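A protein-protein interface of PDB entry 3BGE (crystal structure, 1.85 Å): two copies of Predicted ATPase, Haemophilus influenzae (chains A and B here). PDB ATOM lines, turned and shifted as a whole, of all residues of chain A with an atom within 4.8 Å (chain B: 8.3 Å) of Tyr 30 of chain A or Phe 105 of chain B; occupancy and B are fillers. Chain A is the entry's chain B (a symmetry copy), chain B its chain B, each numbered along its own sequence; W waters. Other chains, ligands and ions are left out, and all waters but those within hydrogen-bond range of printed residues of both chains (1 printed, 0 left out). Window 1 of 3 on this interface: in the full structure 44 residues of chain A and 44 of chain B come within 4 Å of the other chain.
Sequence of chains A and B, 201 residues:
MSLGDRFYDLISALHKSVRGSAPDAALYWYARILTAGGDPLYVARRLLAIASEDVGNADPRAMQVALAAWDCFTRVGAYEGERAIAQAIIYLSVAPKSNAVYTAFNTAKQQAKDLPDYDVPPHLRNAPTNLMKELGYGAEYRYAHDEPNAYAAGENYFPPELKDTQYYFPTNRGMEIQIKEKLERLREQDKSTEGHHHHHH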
ATOM      1  N   LEU A  14       1.931 -28.922  -2.389  1.00  0.00           N
ATOM      2  CA  LEU A  14       3.205 -29.643  -2.423  1.00  0.00           C
ATOM      3  C   LEU A  14       3.275 -30.699  -1.313  1.00  0.00           C
ATOM      4  O   LEU A  14       3.604 -31.867  -1.577  1.00  0.00           O
ATOM      5  CB  LEU A  14       4.396 -28.660  -2.345  1.00  0.00           C
ATOM      6  CG  LEU A  14       5.830 -29.202  -2.119  1.00  0.00           C
ATOM      7  CD1 LEU A  14       6.162 -30.357  -2.984  1.00  0.00           C
ATOM      8  CD2 LEU A  14       6.840 -28.083  -2.347  1.00  0.00           C
ATOM      9  N   ALA A  26       4.360 -33.172  -6.978  1.00  0.00           N
ATOM     10  CA  ALA A  26       5.215 -32.439  -6.009  1.00  0.00           C
ATOM     11  C   ALA A  26       6.198 -31.509  -6.730  1.00  0.00           C
ATOM     12  O   ALA A  26       6.411 -30.342  -6.330  1.00  0.00           O
ATOM     13  CB  ALA A  26       5.980 -33.429  -5.127  1.00  0.00           C
ATOM     14  N   LEU A  27       6.785 -32.018  -7.808  1.00  0.00           N
ATOM     15  CA  LEU A  27       7.710 -31.221  -8.615  1.00  0.00           C
ATOM     16  C   LEU A  27       6.959 -30.051  -9.270  1.00  0.00           C
ATOM     17  O   LEU A  27       7.464 -28.919  -9.304  1.00  0.00           O
ATOM     18  CB  LEU A  27       8.387 -32.098  -9.671  1.00  0.00           C
ATOM     19  CG  LEU A  27       9.535 -33.030  -9.276  1.00  0.00           C
ATOM     20  CD1 LEU A  27       9.966 -33.839 -10.506  1.00  0.00           C
ATOM     21  CD2 LEU A  27      10.720 -32.284  -8.647  1.00  0.00           C
ATOM     22  N   TYR A  28       5.746 -30.312  -9.782  1.00  0.00           N
ATOM     23  CA  TYR A  28       4.897 -29.228 -10.299  1.00  0.00           C
ATOM     24  C   TYR A  28       4.658 -28.079  -9.290  1.00  0.00           C
ATOM     25  O   TYR A  28       4.966 -26.904  -9.579  1.00  0.00           O
ATOM     26  CB  TYR A  28       3.559 -29.762 -10.923  1.00  0.00           C
ATOM     27  CG  TYR A  28       2.632 -28.639 -11.374  1.00  0.00           C
ATOM     28  CD1 TYR A  28       2.793 -28.037 -12.620  1.00  0.00           C
ATOM     29  CD2 TYR A  28       1.610 -28.170 -10.542  1.00  0.00           C
ATOM     30  CE1 TYR A  28       1.943 -26.978 -13.031  1.00  0.00           C
ATOM     31  CE2 TYR A  28       0.768 -27.121 -10.942  1.00  0.00           C
ATOM     32  CZ  TYR A  28       0.952 -26.538 -12.192  1.00  0.00           C
ATOM     33  OH  TYR A  28       0.140 -25.502 -12.582  1.00  0.00           O
ATOM     34  N   TRP A  29       4.178 -28.404  -8.090  1.00  0.00           N
ATOM     35  CA  TRP A  29       3.918 -27.391  -7.076  1.00  0.00           C
ATOM     36  C   TRP A  29       5.185 -26.692  -6.627  1.00  0.00           C
ATOM     37  O   TRP A  29       5.173 -25.490  -6.370  1.00  0.00           O
ATOM     38  CB  TRP A  29       3.117 -27.982  -5.904  1.00  0.00           C
ATOM     39  CG  TRP A  29       1.716 -28.428  -6.405  1.00  0.00           C
ATOM     40  CD1 TRP A  29       1.229 -29.709  -6.471  1.00  0.00           C
ATOM     41  CD2 TRP A  29       0.686 -27.581  -6.951  1.00  0.00           C
ATOM     42  NE1 TRP A  29      -0.048 -29.700  -6.999  1.00  0.00           N
ATOM     43  CE2 TRP A  29      -0.400 -28.413  -7.305  1.00  0.00           C
ATOM     44  CE3 TRP A  29       0.580 -26.201  -7.170  1.00  0.00           C
ATOM     45  CZ2 TRP A  29      -1.586 -27.907  -7.858  1.00  0.00           C
ATOM     46  CZ3 TRP A  29      -0.599 -25.687  -7.707  1.00  0.00           C
ATOM     47  CH2 TRP A  29      -1.677 -26.549  -8.048  1.00  0.00           C
ATOM     48  N   TYR A  30       6.272 -27.452  -6.520  1.00  0.00           N
ATOM     49  CA  TYR A  30       7.596 -26.867  -6.236  1.00  0.00           C
ATOM     50  C   TYR A  30       7.962 -25.849  -7.323  1.00  0.00           C
ATOM     51  O   TYR A  30       8.315 -24.697  -7.023  1.00  0.00           O
ATOM     52  CB  TYR A  30       8.647 -27.977  -6.136  1.00  0.00           C
ATOM     53  CG  TYR A  30      10.074 -27.500  -5.920  1.00  0.00           C
ATOM     54  CD1 TYR A  30      10.370 -26.494  -4.999  1.00  0.00           C
ATOM     55  CD2 TYR A  30      11.144 -28.086  -6.639  1.00  0.00           C
ATOM     56  CE1 TYR A  30      11.703 -26.067  -4.791  1.00  0.00           C
ATOM     57  CE2 TYR A  30      12.468 -27.667  -6.437  1.00  0.00           C
ATOM     58  CZ  TYR A  30      12.732 -26.675  -5.517  1.00  0.00           C
ATOM     59  OH  TYR A  30      14.019 -26.289  -5.336  1.00  0.00           O
ATOM     60  N   ALA A  31       7.909 -26.270  -8.576  1.00  0.00           N
ATOM     61  CA  ALA A  31       8.131 -25.343  -9.729  1.00  0.00           C
ATOM     62  C   ALA A  31       7.223 -24.096  -9.683  1.00  0.00           C
ATOM     63  O   ALA A  31       7.647 -22.957  -9.986  1.00  0.00           O
ATOM     64  CB  ALA A  31       7.925 -26.100 -11.023  1.00  0.00           C
ATOM     65  N   ARG A  32       5.962 -24.297  -9.299  1.00  0.00           N
ATOM     66  CA  ARG A  32       5.021 -23.183  -9.224  1.00  0.00           C
ATOM     67  C   ARG A  32       5.464 -22.160  -8.189  1.00  0.00           C
ATOM     68  O   ARG A  32       5.431 -20.959  -8.446  1.00  0.00           O
ATOM     69  CB  ARG A  32       3.615 -23.684  -8.899  1.00  0.00           C
ATOM     70  CG  ARG A  32       2.908 -24.327 -10.114  1.00  0.00           C
ATOM     71  CD  ARG A  32       2.557 -23.295 -11.220  1.00  0.00           C
ATOM     72  NE  ARG A  32       1.687 -22.224 -10.726  1.00  0.00           N
ATOM     73  CZ  ARG A  32       0.373 -22.327 -10.500  1.00  0.00           C
ATOM     74  NH1 ARG A  32      -0.273 -23.463 -10.693  1.00  0.00           N
ATOM     75  NH2 ARG A  32      -0.289 -21.282 -10.019  1.00  0.00           N
ATOM     76  N   ILE A  33       5.903 -22.648  -7.032  1.00  0.00           N
ATOM     77  CA  ILE A  33       6.402 -21.773  -5.974  1.00  0.00           C
ATOM     78  C   ILE A  33       7.597 -20.953  -6.449  1.00  0.00           C
ATOM     79  O   ILE A  33       7.647 -19.735  -6.232  1.00  0.00           O
ATOM     80  CB  ILE A  33       6.773 -22.579  -4.683  1.00  0.00           C
ATOM     81  CG1 ILE A  33       5.507 -23.136  -4.045  1.00  0.00           C
ATOM     82  CG2 ILE A  33       7.556 -21.674  -3.670  1.00  0.00           C
ATOM     83  CD1 ILE A  33       5.733 -24.256  -3.024  1.00  0.00           C
ATOM     84  N   LEU A  34       8.560 -21.612  -7.093  1.00  0.00           N
ATOM     85  CA  LEU A  34       9.783 -20.914  -7.511  1.00  0.00           C
ATOM     86  C   LEU A  34       9.413 -19.865  -8.556  1.00  0.00           C
ATOM     87  O   LEU A  34       9.842 -18.694  -8.477  1.00  0.00           O
ATOM     88  CB  LEU A  34      10.776 -21.903  -8.114  1.00  0.00           C
ATOM     89  CG  LEU A  34      11.318 -22.951  -7.144  1.00  0.00           C
ATOM     90  CD1 LEU A  34      12.119 -23.947  -7.929  1.00  0.00           C
ATOM     91  CD2 LEU A  34      12.147 -22.252  -6.013  1.00  0.00           C
ATOM     92  N   PRO A  40      13.721 -20.947  -2.473  1.00  0.00           N
ATOM     93  CA  PRO A  40      14.020 -22.367  -2.326  1.00  0.00           C
ATOM     94  C   PRO A  40      14.161 -22.807  -0.853  1.00  0.00           C
ATOM     95  O   PRO A  40      13.844 -23.944  -0.540  1.00  0.00           O
ATOM     96  CB  PRO A  40      15.364 -22.495  -3.029  1.00  0.00           C
ATOM     97  CG  PRO A  40      15.288 -21.417  -4.089  1.00  0.00           C
ATOM     98  CD  PRO A  40      14.736 -20.278  -3.315  1.00  0.00           C
ATOM     99  N   VAL A  43      10.861 -23.513   0.940  1.00  0.00           N
ATOM    100  CA  VAL A  43      10.466 -24.896   0.651  1.00  0.00           C
ATOM    101  C   VAL A  43      11.348 -25.886   1.427  1.00  0.00           C
ATOM    102  O   VAL A  43      10.821 -26.818   2.042  1.00  0.00           O
ATOM    103  CB  VAL A  43      10.545 -25.230  -0.888  1.00  0.00           C
ATOM    104  CG1 VAL A  43      10.255 -26.729  -1.145  1.00  0.00           C
ATOM    105  CG2 VAL A  43       9.629 -24.357  -1.728  1.00  0.00           C
ATOM    106  N   GLY A  81      21.292 -25.568  -5.850  1.00  0.00           N
ATOM    107  CA  GLY A  81      20.449 -25.741  -4.667  1.00  0.00           C
ATOM    108  C   GLY A  81      19.046 -26.188  -5.030  1.00  0.00           C
ATOM    109  O   GLY A  81      18.548 -27.178  -4.490  1.00  0.00           O
ATOM    110  N   GLU A  82      18.422 -25.472  -5.969  1.00  0.00           N
ATOM    111  CA  GLU A  82      17.081 -25.807  -6.484  1.00  0.00           C
ATOM    112  C   GLU A  82      16.974 -27.255  -6.933  1.00  0.00           C
ATOM    113  O   GLU A  82      16.022 -27.958  -6.582  1.00  0.00           O
ATOM    114  CB  GLU A  82      16.753 -24.916  -7.686  1.00  0.00           C
ATOM    115  CG  GLU A  82      16.003 -23.699  -7.320  1.00  0.00           C
ATOM    116  CD  GLU A  82      15.669 -22.850  -8.540  1.00  0.00           C
ATOM    117  OE1 GLU A  82      15.747 -23.333  -9.708  1.00  0.00           O
ATOM    118  OE2 GLU A  82      15.367 -21.671  -8.309  1.00  0.00           O
ATOM    119  N   ARG A  83      17.960 -27.675  -7.704  1.00  0.00           N
ATOM    120  CA  ARG A  83      18.079 -29.044  -8.206  1.00  0.00           C
ATOM    121  C   ARG A  83      18.258 -30.062  -7.087  1.00  0.00           C
ATOM    122  O   ARG A  83      17.627 -31.087  -7.110  1.00  0.00           O
ATOM    123  CB  ARG A  83      19.214 -29.198  -9.221  1.00  0.00           C
ATOM    124  CG  ARG A  83      18.800 -28.904 -10.642  1.00  0.00           C
ATOM    125  CD  ARG A  83      19.352 -27.604 -11.148  1.00  0.00           C
ATOM    126  NE  ARG A  83      18.616 -27.123 -12.323  1.00  0.00           N
ATOM    127  CZ  ARG A  83      18.012 -25.930 -12.416  1.00  0.00           C
ATOM    128  NH1 ARG A  83      18.054 -25.045 -11.404  1.00  0.00           N
ATOM    129  NH2 ARG A  83      17.364 -25.614 -13.541  1.00  0.00           N
ATOM    130  N   ILE A  85      17.257 -29.706  -3.943  1.00  0.00           N
ATOM    131  CA  ILE A  85      15.976 -29.692  -3.224  1.00  0.00           C
ATOM    132  C   ILE A  85      14.903 -30.461  -4.029  1.00  0.00           C
ATOM    133  O   ILE A  85      14.065 -31.166  -3.448  1.00  0.00           O
ATOM    134  CB  ILE A  85      15.541 -28.237  -2.900  1.00  0.00           C
ATOM    135  CG1 ILE A  85      16.500 -27.640  -1.877  1.00  0.00           C
ATOM    136  CG2 ILE A  85      14.090 -28.155  -2.355  1.00  0.00           C
ATOM    137  CD1 ILE A  85      16.414 -26.111  -1.804  1.00  0.00           C
ATOM    138  N   ALA A  86      14.960 -30.370  -5.365  1.00  0.00           N
ATOM    139  CA  ALA A  86      14.100 -31.236  -6.198  1.00  0.00           C
ATOM    140  C   ALA A  86      14.352 -32.721  -5.963  1.00  0.00           C
ATOM    141  O   ALA A  86      13.398 -33.509  -5.812  1.00  0.00           O
ATOM    142  CB  ALA A  86      14.218 -30.894  -7.667  1.00  0.00           C
ATOM    143  N   ILE A  89      12.766 -33.586  -2.768  1.00  0.00           N
ATOM    144  CA  ILE A  89      11.293 -33.697  -2.915  1.00  0.00           C
ATOM    145  C   ILE A  89      10.928 -35.069  -3.453  1.00  0.00           C
ATOM    146  O   ILE A  89      10.008 -35.737  -2.946  1.00  0.00           O
ATOM    147  CB  ILE A  89      10.722 -32.546  -3.802  1.00  0.00           C
ATOM    148  CG1 ILE A  89      10.845 -31.253  -3.024  1.00  0.00           C
ATOM    149  CG2 ILE A  89       9.211 -32.778  -4.175  1.00  0.00           C
ATOM    150  CD1 ILE A  89      10.528 -29.950  -3.877  1.00  0.00           C
ATOM    151  N   SER B  52      23.831 -34.322  -8.492  1.00  0.00           N
ATOM    152  CA  SER B  52      22.429 -33.994  -8.770  1.00  0.00           C
ATOM    153  C   SER B  52      22.036 -34.335 -10.189  1.00  0.00           C
ATOM    154  O   SER B  52      20.948 -34.857 -10.438  1.00  0.00           O
ATOM    155  CB  SER B  52      22.162 -32.511  -8.526  1.00  0.00           C
ATOM    156  OG  SER B  52      22.402 -32.201  -7.165  1.00  0.00           O
ATOM    157  N   ASN B  99      19.987 -39.670 -14.834  1.00  0.00           N
ATOM    158  CA  ASN B  99      19.620 -38.268 -14.867  1.00  0.00           C
ATOM    159  C   ASN B  99      18.104 -38.015 -14.758  1.00  0.00           C
ATOM    160  O   ASN B  99      17.619 -36.963 -15.181  1.00  0.00           O
ATOM    161  CB  ASN B  99      20.264 -37.523 -16.041  1.00  0.00           C
ATOM    162  CG  ASN B  99      19.687 -37.901 -17.365  1.00  0.00           C
ATOM    163  OD1 ASN B  99      19.045 -38.943 -17.513  1.00  0.00           O
ATOM    164  ND2 ASN B  99      19.907 -37.047 -18.357  1.00  0.00           N
ATOM    165  N   ALA B 100      17.361 -38.970 -14.195  1.00  0.00           N
ATOM    166  CA  ALA B 100      15.892 -38.863 -14.172  1.00  0.00           C
ATOM    167  C   ALA B 100      15.389 -37.706 -13.301  1.00  0.00           C
ATOM    168  O   ALA B 100      14.392 -37.054 -13.626  1.00  0.00           O
ATOM    169  CB  ALA B 100      15.239 -40.190 -13.772  1.00  0.00           C
ATOM    170  N   VAL B 101      16.068 -37.438 -12.186  1.00  0.00           N
ATOM    171  CA  VAL B 101      15.562 -36.405 -11.302  1.00  0.00           C
ATOM    172  C   VAL B 101      15.888 -35.066 -11.978  1.00  0.00           C
ATOM    173  O   VAL B 101      15.063 -34.162 -12.025  1.00  0.00           O
ATOM    174  CB  VAL B 101      16.151 -36.489  -9.843  1.00  0.00           C
ATOM    175  CG1 VAL B 101      15.915 -35.165  -9.081  1.00  0.00           C
ATOM    176  CG2 VAL B 101      15.552 -37.654  -9.075  1.00  0.00           C
ATOM    177  N   TYR B 102      17.103 -34.961 -12.507  1.00  0.00           N
ATOM    178  CA  TYR B 102      17.537 -33.760 -13.221  1.00  0.00           C
ATOM    179  C   TYR B 102      16.532 -33.348 -14.302  1.00  0.00           C
ATOM    180  O   TYR B 102      16.037 -32.203 -14.323  1.00  0.00           O
ATOM    181  CB  TYR B 102      18.913 -34.008 -13.861  1.00  0.00           C
ATOM    182  CG  TYR B 102      19.552 -32.791 -14.487  1.00  0.00           C
ATOM    183  CD1 TYR B 102      19.953 -31.718 -13.690  1.00  0.00           C
ATOM    184  CD2 TYR B 102      19.761 -32.707 -15.864  1.00  0.00           C
ATOM    185  CE1 TYR B 102      20.535 -30.606 -14.230  1.00  0.00           C
ATOM    186  CE2 TYR B 102      20.341 -31.571 -16.424  1.00  0.00           C
ATOM    187  CZ  TYR B 102      20.720 -30.529 -15.586  1.00  0.00           C
ATOM    188  OH  TYR B 102      21.312 -29.391 -16.088  1.00  0.00           O
ATOM    189  N   THR B 103      16.231 -34.273 -15.203  1.00  0.00           N
ATOM    190  CA  THR B 103      15.356 -33.919 -16.328  1.00  0.00           C
ATOM    191  C   THR B 103      13.898 -33.702 -15.895  1.00  0.00           C
ATOM    192  O   THR B 103      13.200 -32.868 -16.484  1.00  0.00           O
ATOM    193  CB  THR B 103      15.449 -34.915 -17.472  1.00  0.00           C
ATOM    194  OG1 THR B 103      14.990 -36.189 -17.033  1.00  0.00           O
ATOM    195  CG2 THR B 103      16.886 -35.057 -17.914  1.00  0.00           C
ATOM    196  N   ALA B 104      13.455 -34.428 -14.864  1.00  0.00           N
ATOM    197  CA  ALA B 104      12.119 -34.235 -14.310  1.00  0.00           C
ATOM    198  C   ALA B 104      11.971 -32.800 -13.777  1.00  0.00           C
ATOM    199  O   ALA B 104      11.007 -32.084 -14.100  1.00  0.00           O
ATOM    200  CB  ALA B 104      11.838 -35.271 -13.205  1.00  0.00           C
ATOM    201  N   PHE B 105      12.952 -32.344 -12.997  1.00  0.00           N
ATOM    202  CA  PHE B 105      12.845 -31.003 -12.446  1.00  0.00           C
ATOM    203  C   PHE B 105      12.827 -29.956 -13.561  1.00  0.00           C
ATOM    204  O   PHE B 105      12.057 -28.989 -13.490  1.00  0.00           O
ATOM    205  CB  PHE B 105      13.956 -30.686 -11.422  1.00  0.00           C
ATOM    206  CG  PHE B 105      13.904 -29.256 -10.902  1.00  0.00           C
ATOM    207  CD1 PHE B 105      12.775 -28.772 -10.263  1.00  0.00           C
ATOM    208  CD2 PHE B 105      14.964 -28.395 -11.112  1.00  0.00           C
ATOM    209  CE1 PHE B 105      12.711 -27.447  -9.790  1.00  0.00           C
ATOM    210  CE2 PHE B 105      14.903 -27.102 -10.686  1.00  0.00           C
ATOM    211  CZ  PHE B 105      13.773 -26.617 -10.021  1.00  0.00           C
ATOM    212  N   ASN B 106      13.695 -30.119 -14.562  1.00  0.00           N
ATOM    213  CA  ASN B 106      13.818 -29.148 -15.646  1.00  0.00           C
ATOM    214  C   ASN B 106      12.505 -29.001 -16.402  1.00  0.00           C
ATOM    215  O   ASN B 106      12.092 -27.893 -16.736  1.00  0.00           O
ATOM    216  CB  ASN B 106      14.938 -29.545 -16.634  1.00  0.00           C
ATOM    217  CG  ASN B 106      16.326 -29.337 -16.051  1.00  0.00           C
ATOM    218  OD1 ASN B 106      16.505 -28.632 -15.041  1.00  0.00           O
ATOM    219  ND2 ASN B 106      17.315 -29.926 -16.691  1.00  0.00           N
ATOM    220  N   THR B 107      11.872 -30.136 -16.683  1.00  0.00           N
ATOM    221  CA  THR B 107      10.550 -30.132 -17.287  1.00  0.00           C
ATOM    222  C   THR B 107       9.495 -29.432 -16.441  1.00  0.00           C
ATOM    223  O   THR B 107       8.749 -28.585 -16.942  1.00  0.00           O
ATOM    224  CB  THR B 107      10.064 -31.568 -17.579  1.00  0.00           C
ATOM    225  OG1 THR B 107      11.081 -32.263 -18.304  1.00  0.00           O
ATOM    226  CG2 THR B 107       8.753 -31.541 -18.396  1.00  0.00           C
ATOM    227  N   ALA B 108       9.437 -29.780 -15.159  1.00  0.00           N
ATOM    228  CA  ALA B 108       8.450 -29.190 -14.266  1.00  0.00           C
ATOM    229  C   ALA B 108       8.624 -27.688 -14.253  1.00  0.00           C
ATOM    230  O   ALA B 108       7.632 -26.930 -14.297  1.00  0.00           O
ATOM    231  CB  ALA B 108       8.565 -29.771 -12.826  1.00  0.00           C
ATOM    232  N   LYS B 109       9.879 -27.246 -14.196  1.00  0.00           N
ATOM    233  CA  LYS B 109      10.165 -25.823 -14.082  1.00  0.00           C
ATOM    234  C   LYS B 109       9.778 -25.063 -15.356  1.00  0.00           C
ATOM    235  O   LYS B 109       9.215 -23.963 -15.271  1.00  0.00           O
ATOM    236  CB  LYS B 109      11.630 -25.621 -13.739  1.00  0.00           C
ATOM    237  CG  LYS B 109      11.958 -24.267 -13.168  1.00  0.00           C
ATOM    238  CD  LYS B 109      13.462 -24.210 -12.935  1.00  0.00           C
ATOM    239  CE  LYS B 109      13.963 -22.789 -13.051  1.00  0.00           C
ATOM    240  NZ  LYS B 109      13.490 -21.983 -11.911  1.00  0.00           N
ATOM    241  N   GLN B 110      10.057 -25.654 -16.525  1.00  0.00           N
ATOM    242  CA  GLN B 110       9.693 -25.032 -17.796  1.00  0.00           C
ATOM    243  C   GLN B 110       8.168 -24.964 -17.920  1.00  0.00           C
ATOM    244  O   GLN B 110       7.628 -23.916 -18.256  1.00  0.00           O
ATOM    245  CB  GLN B 110      10.339 -25.721 -18.996  1.00  0.00           C
ATOM    246  CG  GLN B 110      10.201 -24.923 -20.266  1.00  0.00           C
ATOM    247  CD  GLN B 110      10.831 -23.548 -20.101  1.00  0.00           C
ATOM    248  OE1 GLN B 110      10.266 -22.526 -20.507  1.00  0.00           O
ATOM    249  NE2 GLN B 110      11.980 -23.509 -19.429  1.00  0.00           N
ATOM    250  N   GLN B 111       7.469 -26.036 -17.554  1.00  0.00           N
ATOM    251  CA  GLN B 111       5.982 -26.014 -17.542  1.00  0.00           C
ATOM    252  C   GLN B 111       5.401 -24.948 -16.596  1.00  0.00           C
ATOM    253  O   GLN B 111       4.490 -24.199 -16.974  1.00  0.00           O
ATOM    254  CB  GLN B 111       5.410 -27.402 -17.260  1.00  0.00           C
ATOM    255  CG  GLN B 111       5.568 -28.325 -18.459  1.00  0.00           C
ATOM    256  CD  GLN B 111       4.791 -29.594 -18.327  1.00  0.00           C
ATOM    257  OE1 GLN B 111       4.935 -30.498 -19.156  1.00  0.00           O
ATOM    258  NE2 GLN B 111       3.934 -29.679 -17.312  1.00  0.00           N
ATOM    259  N   ALA B 112       5.955 -24.807 -15.399  1.00  0.00           N
ATOM    260  CA  ALA B 112       5.496 -23.735 -14.501  1.00  0.00           C
ATOM    261  C   ALA B 112       5.642 -22.362 -15.153  1.00  0.00           C
ATOM    262  O   ALA B 112       4.809 -21.478 -14.956  1.00  0.00           O
ATOM    263  CB  ALA B 112       6.266 -23.760 -13.142  1.00  0.00           C
ATOM    264  N   LYS B 113       6.710 -22.176 -15.915  1.00  0.00           N
ATOM    265  CA  LYS B 113       6.981 -20.867 -16.501  1.00  0.00           C
ATOM    266  C   LYS B 113       5.994 -20.580 -17.599  1.00  0.00           C
ATOM    267  O   LYS B 113       5.554 -19.451 -17.739  1.00  0.00           O
ATOM    268  CB  LYS B 113       8.407 -20.788 -17.054  1.00  0.00           C
ATOM    269  CG  LYS B 113       9.458 -20.741 -15.961  1.00  0.00           C
ATOM    270  CD  LYS B 113      10.849 -20.550 -16.543  1.00  0.00           C
ATOM    271  CE  LYS B 113      11.905 -20.982 -15.544  1.00  0.00           C
ATOM    272  NZ  LYS B 113      13.275 -20.703 -16.057  1.00  0.00           N
ATOM    273  N   TYR B 167       6.663 -36.314 -15.028  1.00  0.00           N
ATOM    274  CA  TYR B 167       7.988 -35.741 -15.299  1.00  0.00           C
ATOM    275  C   TYR B 167       9.102 -36.749 -15.003  1.00  0.00           C
ATOM    276  O   TYR B 167      10.140 -36.760 -15.676  1.00  0.00           O
ATOM    277  CB  TYR B 167       8.222 -34.545 -14.400  1.00  0.00           C
ATOM    278  CG  TYR B 167       7.217 -33.430 -14.545  1.00  0.00           C
ATOM    279  CD1 TYR B 167       6.861 -32.926 -15.797  1.00  0.00           C
ATOM    280  CD2 TYR B 167       6.601 -32.883 -13.416  1.00  0.00           C
ATOM    281  CE1 TYR B 167       5.968 -31.869 -15.916  1.00  0.00           C
ATOM    282  CE2 TYR B 167       5.690 -31.835 -13.533  1.00  0.00           C
ATOM    283  CZ  TYR B 167       5.393 -31.332 -14.775  1.00  0.00           C
ATOM    284  OH  TYR B 167       4.476 -30.300 -14.855  1.00  0.00           O
ATOM    285  N   TYR B 168       8.885 -37.566 -13.967  1.00  0.00           N
ATOM    286  CA  TYR B 168       9.910 -38.442 -13.417  1.00  0.00           C
ATOM    287  C   TYR B 168       9.828 -39.880 -13.946  1.00  0.00           C
ATOM    288  O   TYR B 168       8.856 -40.608 -13.671  1.00  0.00           O
ATOM    289  CB  TYR B 168       9.795 -38.436 -11.896  1.00  0.00           C
ATOM    290  CG  TYR B 168      10.857 -39.239 -11.165  1.00  0.00           C
ATOM    291  CD1 TYR B 168      12.224 -39.077 -11.450  1.00  0.00           C
ATOM    292  CD2 TYR B 168      10.498 -40.139 -10.172  1.00  0.00           C
ATOM    293  CE1 TYR B 168      13.202 -39.825 -10.775  1.00  0.00           C
ATOM    294  CE2 TYR B 168      11.459 -40.852  -9.479  1.00  0.00           C
ATOM    295  CZ  TYR B 168      12.804 -40.717  -9.805  1.00  0.00           C
ATOM    296  OH  TYR B 168      13.760 -41.437  -9.088  1.00  0.00           O
HETATM  297  O   HOH W   1      14.115 -20.028  -9.634  1.00  0.00           O
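The side-chain amide oxygen (OD1) of Asn 106 of chain B lies within hydrogen-bond range of the guanidinium group (NH2) of Arg 83 of chain A, 3.5 Å away.
The side-chain amino group (NZ) of Lys 109 of chain B lies within salt-bridge range of the side-chain carboxylate (OE1) of Glu 82 of chain A, 3.4 Å away.
The side-chain amide nitrogen of Gln 111 of chain B sits at hydrogen-bond distance from the side-chain hydroxyl of Tyr 167 of chain B (2.6 Å).
NH1 of Arg 32 of chain A lies within hydrogen-bond range of OH of Tyr 28 of chain A (2.8 Å).
OH of Tyr 30 of chain A is in hydrogen-bond range of O of Glu 82 of chain A (2.9 Å).
The guanidinium group (NH1) of Arg 83 of chain A is in salt-bridge range of the side-chain carboxylate (OE1) of Glu 82 of chain A (3.3 Å).
CB of Ala 108 of chain B touches O of Leu 27 of chain A (3.8 Å).
CD1 of Tyr 28 of chain A touches OH of Tyr 167 of chain B (3.6 Å).
CE1 of Phe 105 of chain B touches CE2 of Tyr 30 of chain A, 3.4 Å away.
Ala 31 of chain A touches Ala 108 of chain B (CB to O, 3.4 Å).
CA of Lys 109 of chain B touches CB of Ala 31 of chain A, 3.8 Å away.
Ala 112 of chain B touches Ala 31 of chain A (CB to O, 3.5 Å).
Arg 32 of chain A touches Ala 112 of chain B (N to CB, 3.9 Å).
Phe 105 of chain B touches Leu 34 of chain A (CZ to CD1, 3.8 Å).
Arg 83 of chain A touches Phe 105 of chain B (CZ to CE2, 3.7 Å).
CB of Ala 86 of chain A touches CG of Phe 105 of chain B, at 3.6 Å.
Tyr 30 of chain A touches one residue of chain B.
Of chain B, only Ala 108 (3.4 Å), Lys 109 (3.8 Å) and Ala 112 (3.5 Å) come within 4 Å of Ala 31 of chain A.
Printed residues of chain B within 4 Å of Glu 82 of chain A: Phe 105 and Lys 109.
Of the printed residues of chain B, Arg 83 of chain A touches Phe 105 and Asn 106.
Of the printed residues of chain B, Ala 86 of chain A touches Phe 105 (3.6 Å).
Printed residues of chain A within 4 Å of Ala 104 of chain B: Leu 27 (3.6 Å).
Of chain A, only Tyr 30, Leu 34, Glu 82, Arg 83 and Ala 86 come within 4 Å of Phe 105 of chain B.
Of the printed residues of chain A, Ala 112 of chain B touches Ala 31 (3.5 Å) and Arg 32 (3.9 Å).
The nearest residue of chain B that does not touch Tyr 30 of chain A is Ala 112 of chain B (6.4 Å).
The nearest printed residue of chain A that does not touch Lys 109 of chain B is Arg 83 of chain A (4.2 Å).
Hydrophobic or aromatic side chains of chain A within 4 Å of the printed part of chain B: Leu 27, Tyr 28, Tyr 30, Ala 31, Leu 34 and Ala 86.
Among the printed residues, 14 pairs touch across the chains.
No position is printed for both chains.
Of the 14 pairs that touch across the chains among the printed residues, none has its exchanged pair printed and touching as well.
Water W1 bridges the side-chain carboxylate of Glu 82 of chain A (2.5 Å) and the side-chain amino group of Lys 109 of chain B (3.1 Å).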
